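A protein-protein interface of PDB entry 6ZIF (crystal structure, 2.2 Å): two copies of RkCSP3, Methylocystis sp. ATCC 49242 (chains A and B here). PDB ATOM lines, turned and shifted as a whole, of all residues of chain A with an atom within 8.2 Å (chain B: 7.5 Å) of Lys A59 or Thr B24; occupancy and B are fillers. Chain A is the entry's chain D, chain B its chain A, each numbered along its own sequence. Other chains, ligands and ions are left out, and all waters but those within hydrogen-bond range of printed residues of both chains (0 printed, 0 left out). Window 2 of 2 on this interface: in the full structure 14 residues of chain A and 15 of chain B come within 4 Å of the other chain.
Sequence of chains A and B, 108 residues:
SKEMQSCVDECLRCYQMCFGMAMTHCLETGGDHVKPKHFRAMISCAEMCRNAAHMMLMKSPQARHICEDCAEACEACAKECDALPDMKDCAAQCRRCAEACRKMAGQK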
ATOM      1  N   SER A   1      -6.684   2.357  -5.540  1.00  0.00           N
ATOM      2  CA  SER A   1      -7.077   3.786  -5.724  1.00  0.00           C
ATOM      3  C   SER A   1      -6.268   4.674  -4.779  1.00  0.00           C
ATOM      4  O   SER A   1      -5.080   4.425  -4.597  1.00  0.00           O
ATOM      5  CB  SER A   1      -8.554   3.963  -5.557  1.00  0.00           C
ATOM      6  OG  SER A   1      -8.917   3.705  -4.219  1.00  0.00           O
ATOM      7  N   MET A   4      -7.834   4.669  -0.687  1.00  0.00           N
ATOM      8  CA  MET A   4      -7.560   3.327  -0.204  1.00  0.00           C
ATOM      9  C   MET A   4      -6.127   3.239   0.326  1.00  0.00           C
ATOM     10  O   MET A   4      -5.915   2.766   1.441  1.00  0.00           O
ATOM     11  CB  MET A   4      -7.760   2.311  -1.326  1.00  0.00           C
ATOM     12  CG  MET A   4      -7.707   0.880  -0.855  1.00  0.00           C
ATOM     13  SD  MET A   4      -9.210   0.418   0.052  1.00  0.00           S
ATOM     14  CE  MET A   4      -9.415  -1.318  -0.351  1.00  0.00           C
ATOM     15  N   GLN A   5      -5.145   3.689  -0.480  1.00  0.00           N
ATOM     16  CA  GLN A   5      -3.759   3.672  -0.026  1.00  0.00           C
ATOM     17  C   GLN A   5      -3.615   4.612   1.164  1.00  0.00           C
ATOM     18  O   GLN A   5      -2.716   4.459   1.972  1.00  0.00           O
ATOM     19  CB  GLN A   5      -2.764   4.009  -1.131  1.00  0.00           C
ATOM     20  CG  GLN A   5      -2.116   2.771  -1.752  1.00  0.00           C
ATOM     21  CD  GLN A   5      -2.264   2.764  -3.256  1.00  0.00           C
ATOM     22  OE1 GLN A   5      -2.422   3.809  -3.884  1.00  0.00           O
ATOM     23  NE2 GLN A   5      -2.231   1.583  -3.857  1.00  0.00           N
ATOM     24  N   ALA A  52      -7.047  -4.466   9.604  1.00  0.00           N
ATOM     25  CA  ALA A  52      -7.756  -3.692   8.598  1.00  0.00           C
ATOM     26  C   ALA A  52      -6.848  -3.469   7.397  1.00  0.00           C
ATOM     27  O   ALA A  52      -7.299  -3.549   6.260  1.00  0.00           O
ATOM     28  CB  ALA A  52      -8.183  -2.359   9.165  1.00  0.00           C
ATOM     29  N   ALA A  53      -5.568  -3.162   7.646  1.00  0.00           N
ATOM     30  CA  ALA A  53      -4.620  -2.927   6.560  1.00  0.00           C
ATOM     31  C   ALA A  53      -4.557  -4.159   5.654  1.00  0.00           C
ATOM     32  O   ALA A  53      -4.674  -4.061   4.445  1.00  0.00           O
ATOM     33  CB  ALA A  53      -3.271  -2.561   7.122  1.00  0.00           C
ATOM     34  N   HIS A  54      -4.441  -5.330   6.278  1.00  0.00           N
ATOM     35  CA  HIS A  54      -4.362  -6.610   5.607  1.00  0.00           C
ATOM     36  C   HIS A  54      -5.587  -6.840   4.713  1.00  0.00           C
ATOM     37  O   HIS A  54      -5.449  -7.213   3.558  1.00  0.00           O
ATOM     38  CB  HIS A  54      -4.231  -7.706   6.678  1.00  0.00           C
ATOM     39  CG  HIS A  54      -3.505  -8.920   6.224  1.00  0.00           C
ATOM     40  ND1 HIS A  54      -2.179  -8.871   5.852  1.00  0.00           N
ATOM     41  CD2 HIS A  54      -3.871 -10.223   6.151  1.00  0.00           C
ATOM     42  CE1 HIS A  54      -1.758 -10.091   5.555  1.00  0.00           C
ATOM     43  NE2 HIS A  54      -2.781 -10.937   5.713  1.00  0.00           N
ATOM     44  N   MET A  55      -6.792  -6.662   5.277  1.00  0.00           N
ATOM     45  CA  MET A  55      -8.029  -6.929   4.561  1.00  0.00           C
ATOM     46  C   MET A  55      -8.163  -5.955   3.388  1.00  0.00           C
ATOM     47  O   MET A  55      -8.649  -6.327   2.325  1.00  0.00           O
ATOM     48  CB  MET A  55      -9.247  -6.789   5.477  1.00  0.00           C
ATOM     49  CG  MET A  55      -9.273  -7.799   6.626  1.00  0.00           C
ATOM     50  SD  MET A  55      -9.507  -9.496   6.067  1.00  0.00           S
ATOM     51  CE  MET A  55      -7.814 -10.082   5.987  1.00  0.00           C
ATOM     52  N   MET A  56      -7.717  -4.708   3.564  1.00  0.00           N
ATOM     53  CA  MET A  56      -7.742  -3.750   2.474  1.00  0.00           C
ATOM     54  C   MET A  56      -6.750  -4.142   1.384  1.00  0.00           C
ATOM     55  O   MET A  56      -7.078  -4.074   0.205  1.00  0.00           O
ATOM     56  CB  MET A  56      -7.408  -2.342   2.970  1.00  0.00           C
ATOM     57  CG  MET A  56      -8.586  -1.656   3.685  1.00  0.00           C
ATOM     58  SD  MET A  56      -8.140   0.057   4.180  1.00  0.00           S
ATOM     59  CE  MET A  56      -7.085  -0.228   5.606  1.00  0.00           C
ATOM     60  N   LEU A  57      -5.527  -4.549   1.775  1.00  0.00           N
ATOM     61  CA  LEU A  57      -4.478  -4.835   0.809  1.00  0.00           C
ATOM     62  C   LEU A  57      -4.879  -5.982  -0.109  1.00  0.00           C
ATOM     63  O   LEU A  57      -4.419  -6.030  -1.239  1.00  0.00           O
ATOM     64  CB  LEU A  57      -3.177  -5.180   1.542  1.00  0.00           C
ATOM     65  CG  LEU A  57      -2.356  -3.977   2.002  1.00  0.00           C
ATOM     66  CD1 LEU A  57      -1.278  -4.415   2.978  1.00  0.00           C
ATOM     67  CD2 LEU A  57      -1.770  -3.221   0.806  1.00  0.00           C
ATOM     68  N   MET A  58      -5.701  -6.918   0.389  1.00  0.00           N
ATOM     69  CA  MET A  58      -6.092  -8.065  -0.407  1.00  0.00           C
ATOM     70  C   MET A  58      -7.440  -7.820  -1.085  1.00  0.00           C
ATOM     71  O   MET A  58      -8.014  -8.750  -1.654  1.00  0.00           O
ATOM     72  CB  MET A  58      -6.172  -9.326   0.452  1.00  0.00           C
ATOM     73  CG  MET A  58      -7.301  -9.310   1.441  1.00  0.00           C
ATOM     74  SD  MET A  58      -7.376 -10.901   2.302  1.00  0.00           S
ATOM     75  CE  MET A  58      -7.667 -11.912   0.863  1.00  0.00           C
ATOM     76  N   LYS A  59      -7.936  -6.572  -1.017  1.00  0.00           N
ATOM     77  CA  LYS A  59      -9.231  -6.190  -1.562  1.00  0.00           C
ATOM     78  C   LYS A  59     -10.292  -7.184  -1.105  1.00  0.00           C
ATOM     79  O   LYS A  59     -11.058  -7.692  -1.907  1.00  0.00           O
ATOM     80  CB  LYS A  59      -9.206  -6.144  -3.095  1.00  0.00           C
ATOM     81  CG  LYS A  59      -8.269  -5.123  -3.707  1.00  0.00           C
ATOM     82  CD  LYS A  59      -8.391  -5.106  -5.213  1.00  0.00           C
ATOM     83  CE  LYS A  59      -7.583  -3.981  -5.825  1.00  0.00           C
ATOM     84  NZ  LYS A  59      -7.338  -4.221  -7.265  1.00  0.00           N
ATOM     85  N   SER A  60     -10.335  -7.468   0.191  1.00  0.00           N
ATOM     86  CA  SER A  60     -11.361  -8.342   0.727  1.00  0.00           C
ATOM     87  C   SER A  60     -12.748  -7.726   0.540  1.00  0.00           C
ATOM     88  O   SER A  60     -12.914  -6.511   0.651  1.00  0.00           O
ATOM     89  CB  SER A  60     -11.107  -8.610   2.173  1.00  0.00           C
ATOM     90  OG  SER A  60     -12.278  -9.176   2.748  1.00  0.00           O
ATOM     91  N   PRO A  61     -13.783  -8.543   0.249  1.00  0.00           N
ATOM     92  CA  PRO A  61     -15.170  -8.065   0.236  1.00  0.00           C
ATOM     93  C   PRO A  61     -15.574  -7.302   1.496  1.00  0.00           C
ATOM     94  O   PRO A  61     -16.327  -6.354   1.411  1.00  0.00           O
ATOM     95  CB  PRO A  61     -16.002  -9.359   0.205  1.00  0.00           C
ATOM     96  CG  PRO A  61     -15.093 -10.379  -0.431  1.00  0.00           C
ATOM     97  CD  PRO A  61     -13.669  -9.970  -0.087  1.00  0.00           C
ATOM     98  N   GLN A  62     -15.052  -7.707   2.664  1.00  0.00           N
ATOM     99  CA  GLN A  62     -15.477  -7.158   3.947  1.00  0.00           C
ATOM    100  C   GLN A  62     -14.608  -5.983   4.406  1.00  0.00           C
ATOM    101  O   GLN A  62     -14.752  -5.535   5.539  1.00  0.00           O
ATOM    102  CB  GLN A  62     -15.392  -8.234   5.024  1.00  0.00           C
ATOM    103  CG  GLN A  62     -16.302  -9.427   4.822  1.00  0.00           C
ATOM    104  CD  GLN A  62     -16.040 -10.457   5.894  1.00  0.00           C
ATOM    105  OE1 GLN A  62     -16.827 -11.370   6.131  1.00  0.00           O
ATOM    106  NE2 GLN A  62     -14.912 -10.333   6.566  1.00  0.00           N
ATOM    107  N   ALA A  63     -13.726  -5.455   3.542  1.00  0.00           N
ATOM    108  CA  ALA A  63     -12.789  -4.407   3.938  1.00  0.00           C
ATOM    109  C   ALA A  63     -13.516  -3.174   4.457  1.00  0.00           C
ATOM    110  O   ALA A  63     -13.113  -2.606   5.462  1.00  0.00           O
ATOM    111  CB  ALA A  63     -11.825  -4.076   2.827  1.00  0.00           C
ATOM    112  N   ARG A  64     -14.601  -2.779   3.786  1.00  0.00           N
ATOM    113  CA  ARG A  64     -15.376  -1.597   4.141  1.00  0.00           C
ATOM    114  C   ARG A  64     -15.974  -1.758   5.534  1.00  0.00           C
ATOM    115  O   ARG A  64     -15.888  -0.850   6.359  1.00  0.00           O
ATOM    116  CB  ARG A  64     -16.467  -1.330   3.098  1.00  0.00           C
ATOM    117  CG  ARG A  64     -16.156  -0.284   2.037  1.00  0.00           C
ATOM    118  CD  ARG A  64     -17.514   0.071   1.451  1.00  0.00           C
ATOM    119  NE  ARG A  64     -17.459   0.653   0.124  1.00  0.00           N
ATOM    120  CZ  ARG A  64     -18.435   0.562  -0.779  1.00  0.00           C
ATOM    121  NH1 ARG A  64     -19.548  -0.092  -0.496  1.00  0.00           N
ATOM    122  NH2 ARG A  64     -18.298   1.120  -1.974  1.00  0.00           N
ATOM    123  N   GLN B  16       3.700  -4.318   2.238  1.00  0.00           N
ATOM    124  CA  GLN B  16       2.591  -3.796   1.448  1.00  0.00           C
ATOM    125  C   GLN B  16       2.755  -4.186  -0.016  1.00  0.00           C
ATOM    126  O   GLN B  16       1.793  -4.596  -0.679  1.00  0.00           O
ATOM    127  CB  GLN B  16       2.633  -2.271   1.484  1.00  0.00           C
ATOM    128  CG  GLN B  16       1.812  -1.667   2.596  1.00  0.00           C
ATOM    129  CD  GLN B  16       1.561  -0.217   2.274  1.00  0.00           C
ATOM    130  OE1 GLN B  16       0.847   0.131   1.339  1.00  0.00           O
ATOM    131  NE2 GLN B  16       2.174   0.640   3.044  1.00  0.00           N
ATOM    132  N   MET B  17       3.994  -4.040  -0.510  1.00  0.00           N
ATOM    133  CA  MET B  17       4.357  -4.360  -1.875  1.00  0.00           C
ATOM    134  C   MET B  17       4.042  -5.831  -2.153  1.00  0.00           C
ATOM    135  O   MET B  17       3.232  -6.146  -3.022  1.00  0.00           O
ATOM    136  CB  MET B  17       5.849  -4.061  -2.090  1.00  0.00           C
ATOM    137  CG  MET B  17       6.397  -4.497  -3.455  1.00  0.00           C
ATOM    138  SD  MET B  17       5.598  -3.571  -4.793  1.00  0.00           S
ATOM    139  CE  MET B  17       6.552  -2.049  -4.794  1.00  0.00           C
ATOM    140  N   CYS B  18       4.661  -6.745  -1.395  1.00  0.00           N
ATOM    141  CA  CYS B  18       4.579  -8.168  -1.698  1.00  0.00           C
ATOM    142  C   CYS B  18       3.176  -8.725  -1.445  1.00  0.00           C
ATOM    143  O   CYS B  18       2.683  -9.535  -2.226  1.00  0.00           O
ATOM    144  CB  CYS B  18       5.631  -8.926  -0.905  1.00  0.00           C
ATOM    145  SG  CYS B  18       7.312  -8.592  -1.521  1.00  0.00           S
ATOM    146  N   PHE B  19       2.524  -8.321  -0.351  1.00  0.00           N
ATOM    147  CA  PHE B  19       1.207  -8.886  -0.073  1.00  0.00           C
ATOM    148  C   PHE B  19       0.154  -8.281  -0.999  1.00  0.00           C
ATOM    149  O   PHE B  19      -0.703  -8.993  -1.518  1.00  0.00           O
ATOM    150  CB  PHE B  19       0.822  -8.752   1.401  1.00  0.00           C
ATOM    151  CG  PHE B  19      -0.496  -9.409   1.707  1.00  0.00           C
ATOM    152  CD1 PHE B  19      -0.611 -10.795   1.739  1.00  0.00           C
ATOM    153  CD2 PHE B  19      -1.634  -8.643   1.938  1.00  0.00           C
ATOM    154  CE1 PHE B  19      -1.841 -11.391   1.988  1.00  0.00           C
ATOM    155  CE2 PHE B  19      -2.859  -9.237   2.199  1.00  0.00           C
ATOM    156  CZ  PHE B  19      -2.957 -10.609   2.225  1.00  0.00           C
ATOM    157  N   GLY B  20       0.242  -6.956  -1.204  1.00  0.00           N
ATOM    158  CA  GLY B  20      -0.669  -6.233  -2.077  1.00  0.00           C
ATOM    159  C   GLY B  20      -0.558  -6.689  -3.529  1.00  0.00           C
ATOM    160  O   GLY B  20      -1.576  -6.869  -4.200  1.00  0.00           O
ATOM    161  N   MET B  21       0.670  -6.874  -4.026  1.00  0.00           N
ATOM    162  CA  MET B  21       0.879  -7.355  -5.388  1.00  0.00           C
ATOM    163  C   MET B  21       0.364  -8.783  -5.550  1.00  0.00           C
ATOM    164  O   MET B  21      -0.341  -9.096  -6.509  1.00  0.00           O
ATOM    165  CB  MET B  21       2.372  -7.342  -5.735  1.00  0.00           C
ATOM    166  CG  MET B  21       2.913  -5.969  -6.057  1.00  0.00           C
ATOM    167  SD  MET B  21       2.330  -5.371  -7.652  1.00  0.00           S
ATOM    168  CE  MET B  21       0.815  -4.527  -7.181  1.00  0.00           C
ATOM    169  N   ALA B  22       0.722  -9.668  -4.604  1.00  0.00           N
ATOM    170  CA  ALA B  22       0.293 -11.046  -4.720  1.00  0.00           C
ATOM    171  C   ALA B  22      -1.226 -11.120  -4.836  1.00  0.00           C
ATOM    172  O   ALA B  22      -1.748 -11.846  -5.684  1.00  0.00           O
ATOM    173  CB  ALA B  22       0.789 -11.845  -3.551  1.00  0.00           C
ATOM    174  N   MET B  23      -1.941 -10.376  -3.991  1.00  0.00           N
ATOM    175  CA  MET B  23      -3.370 -10.620  -3.863  1.00  0.00           C
ATOM    176  C   MET B  23      -4.152  -9.778  -4.870  1.00  0.00           C
ATOM    177  O   MET B  23      -5.354  -9.944  -4.997  1.00  0.00           O
ATOM    178  CB  MET B  23      -3.850 -10.297  -2.447  1.00  0.00           C
ATOM    179  CG  MET B  23      -3.266 -11.249  -1.400  1.00  0.00           C
ATOM    180  SD  MET B  23      -3.636 -13.008  -1.748  1.00  0.00           S
ATOM    181  CE  MET B  23      -5.433 -12.942  -1.725  1.00  0.00           C
ATOM    182  N   THR B  24      -3.474  -8.869  -5.579  1.00  0.00           N
ATOM    183  CA  THR B  24      -4.143  -8.071  -6.596  1.00  0.00           C
ATOM    184  C   THR B  24      -3.570  -8.417  -7.969  1.00  0.00           C
ATOM    185  O   THR B  24      -4.063  -9.348  -8.613  1.00  0.00           O
ATOM    186  CB  THR B  24      -4.245  -6.583  -6.227  1.00  0.00           C
ATOM    187  OG1 THR B  24      -2.914  -6.077  -6.233  1.00  0.00           O
ATOM    188  CG2 THR B  24      -4.889  -6.359  -4.873  1.00  0.00           C
ATOM    189  N   HIS B  25      -2.492  -7.738  -8.374  1.00  0.00           N
ATOM    190  CA  HIS B  25      -1.897  -7.974  -9.678  1.00  0.00           C
ATOM    191  C   HIS B  25      -1.659  -9.459  -9.979  1.00  0.00           C
ATOM    192  O   HIS B  25      -2.110  -9.942 -11.014  1.00  0.00           O
ATOM    193  CB  HIS B  25      -0.647  -7.111  -9.906  1.00  0.00           C
ATOM    194  CG  HIS B  25      -0.006  -7.406 -11.225  1.00  0.00           C
ATOM    195  ND1 HIS B  25      -0.504  -6.887 -12.412  1.00  0.00           N
ATOM    196  CD2 HIS B  25       1.037  -8.207 -11.569  1.00  0.00           C
ATOM    197  CE1 HIS B  25       0.231  -7.318 -13.421  1.00  0.00           C
ATOM    198  NE2 HIS B  25       1.179  -8.131 -12.927  1.00  0.00           N
ATOM    199  N   CYS B  26      -0.909 -10.176  -9.130  1.00  0.00           N
ATOM    200  CA  CYS B  26      -0.534 -11.551  -9.446  1.00  0.00           C
ATOM    201  C   CYS B  26      -1.757 -12.461  -9.519  1.00  0.00           C
ATOM    202  O   CYS B  26      -1.896 -13.243 -10.457  1.00  0.00           O
ATOM    203  CB  CYS B  26       0.449 -12.117  -8.432  1.00  0.00           C
ATOM    204  SG  CYS B  26       1.958 -11.133  -8.375  1.00  0.00           S
ATOM    205  N   LEU B  27      -2.642 -12.376  -8.519  1.00  0.00           N
ATOM    206  CA  LEU B  27      -3.852 -13.191  -8.510  1.00  0.00           C
ATOM    207  C   LEU B  27      -4.700 -12.875  -9.743  1.00  0.00           C
ATOM    208  O   LEU B  27      -5.328 -13.759 -10.301  1.00  0.00           O
ATOM    209  CB  LEU B  27      -4.636 -12.923  -7.227  1.00  0.00           C
ATOM    210  CG  LEU B  27      -5.670 -13.959  -6.797  1.00  0.00           C
ATOM    211  CD1 LEU B  27      -5.077 -15.361  -6.775  1.00  0.00           C
ATOM    212  CD2 LEU B  27      -6.202 -13.628  -5.399  1.00  0.00           C
ATOM    213  N   GLU B  28      -4.737 -11.604 -10.170  1.00  0.00           N
ATOM    214  CA  GLU B  28      -5.625 -11.235 -11.260  1.00  0.00           C
ATOM    215  C   GLU B  28      -5.017 -11.600 -12.607  1.00  0.00           C
ATOM    216  O   GLU B  28      -5.746 -11.836 -13.550  1.00  0.00           O
ATOM    217  CB  GLU B  28      -6.141  -9.806 -11.146  1.00  0.00           C
ATOM    218  CG  GLU B  28      -7.346  -9.767 -10.215  1.00  0.00           C
ATOM    219  CD  GLU B  28      -7.421  -8.609  -9.230  1.00  0.00           C
ATOM    220  OE1 GLU B  28      -6.918  -7.507  -9.563  1.00  0.00           O
ATOM    221  OE2 GLU B  28      -7.942  -8.819  -8.105  1.00  0.00           O
ATOM    222  N   THR B  29      -3.689 -11.632 -12.706  1.00  0.00           N
ATOM    223  CA  THR B  29      -3.041 -11.999 -13.954  1.00  0.00           C
ATOM    224  C   THR B  29      -3.065 -13.518 -14.132  1.00  0.00           C
ATOM    225  O   THR B  29      -3.243 -14.004 -15.243  1.00  0.00           O
ATOM    226  CB  THR B  29      -1.613 -11.447 -14.017  1.00  0.00           C
ATOM    227  OG1 THR B  29      -1.722 -10.039 -13.815  1.00  0.00           O
ATOM    228  CG2 THR B  29      -0.945 -11.701 -15.345  1.00  0.00           C
ATOM    229  N   GLY B  30      -2.850 -14.283 -13.056  1.00  0.00           N
ATOM    230  CA  GLY B  30      -2.692 -15.731 -13.185  1.00  0.00           C
ATOM    231  C   GLY B  30      -1.376 -16.074 -13.890  1.00  0.00           C
ATOM    232  O   GLY B  30      -0.425 -15.272 -13.893  1.00  0.00           O
ATOM    233  N   PHE B  39       4.745 -17.658  -6.005  1.00  0.00           N
ATOM    234  CA  PHE B  39       3.682 -17.064  -5.210  1.00  0.00           C
ATOM    235  C   PHE B  39       3.952 -17.279  -3.722  1.00  0.00           C
ATOM    236  O   PHE B  39       3.745 -16.381  -2.902  1.00  0.00           O
ATOM    237  CB  PHE B  39       2.324 -17.671  -5.576  1.00  0.00           C
ATOM    238  CG  PHE B  39       1.139 -16.897  -5.060  1.00  0.00           C
ATOM    239  CD1 PHE B  39       0.650 -15.800  -5.748  1.00  0.00           C
ATOM    240  CD2 PHE B  39       0.547 -17.224  -3.850  1.00  0.00           C
ATOM    241  CE1 PHE B  39      -0.464 -15.111  -5.283  1.00  0.00           C
ATOM    242  CE2 PHE B  39      -0.544 -16.527  -3.367  1.00  0.00           C
ATOM    243  CZ  PHE B  39      -1.040 -15.463  -4.076  1.00  0.00           C
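The side-chain hydroxyl (OG1) of Thr B24 sits at hydrogen-bond distance from the backbone carbonyl oxygen (O) of Gly B20, 2.6 Å away.
Among the printed residues, pairs that only touch across the chains: His A54 with Phe B19, Met A58 with Met B23, Leu A57 with Thr B24, Lys A59 with Thr B24, Met A58 with Phe B19, Leu A57 with Phe B19 and Leu A57 with Gly B20.
Of the printed residues of chain B, Lys A59 touches Thr B24.
Thr B24 touches just these residues of chain A: Leu A57 and Lys A59.
Of the printed residues of chain B, Met A58 touches Phe B19 (3.7 Å) and Met B23 (3.6 Å).
Of the printed residues of chain B, Leu A57 touches Phe B19, Gly B20 and Thr B24.
Printed residues of chain A within 4 Å of Met B23: Met A58 (3.6 Å).
Of the printed residues of chain B, His A54 touches Phe B19.
Of the printed residues of chain A, Gly B20 touches Leu A57 (3.8 Å).
Gln A5 touches none of the printed residues of chain B.
The nearest residue of chain B that does not touch Lys A59 is Glu B28 (4.03 Å).
The nearest printed residue of chain A that does not touch Gly B20 is Met A58 (5.6 Å).
Of the 16 printed residues of chain A, 4 touch a printed residue of chain B.
Printed residues of chain A that touch a printed residue of chain B: His A54, Leu A57, Met A58 and Lys A59.
Hydrophobic or aromatic side chains of chain A that line the printed part of chain B: His A54, Leu A57 and Met A58.
Printed residues of chain B that touch a printed residue of chain A: Phe B19, Gly B20, Met B23 and Thr B24.
Hydrophobic or aromatic side chains of chain B within 4 Å of the printed part of chain A: Phe B19 and Met B23.
Among the printed residues, 7 pairs touch across the chains.
Among the printed residues, no Asp or Glu carboxylate lies within 4 Å of a Lys or Arg side-chain nitrogen of the other chain.
No position is printed for both chains.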
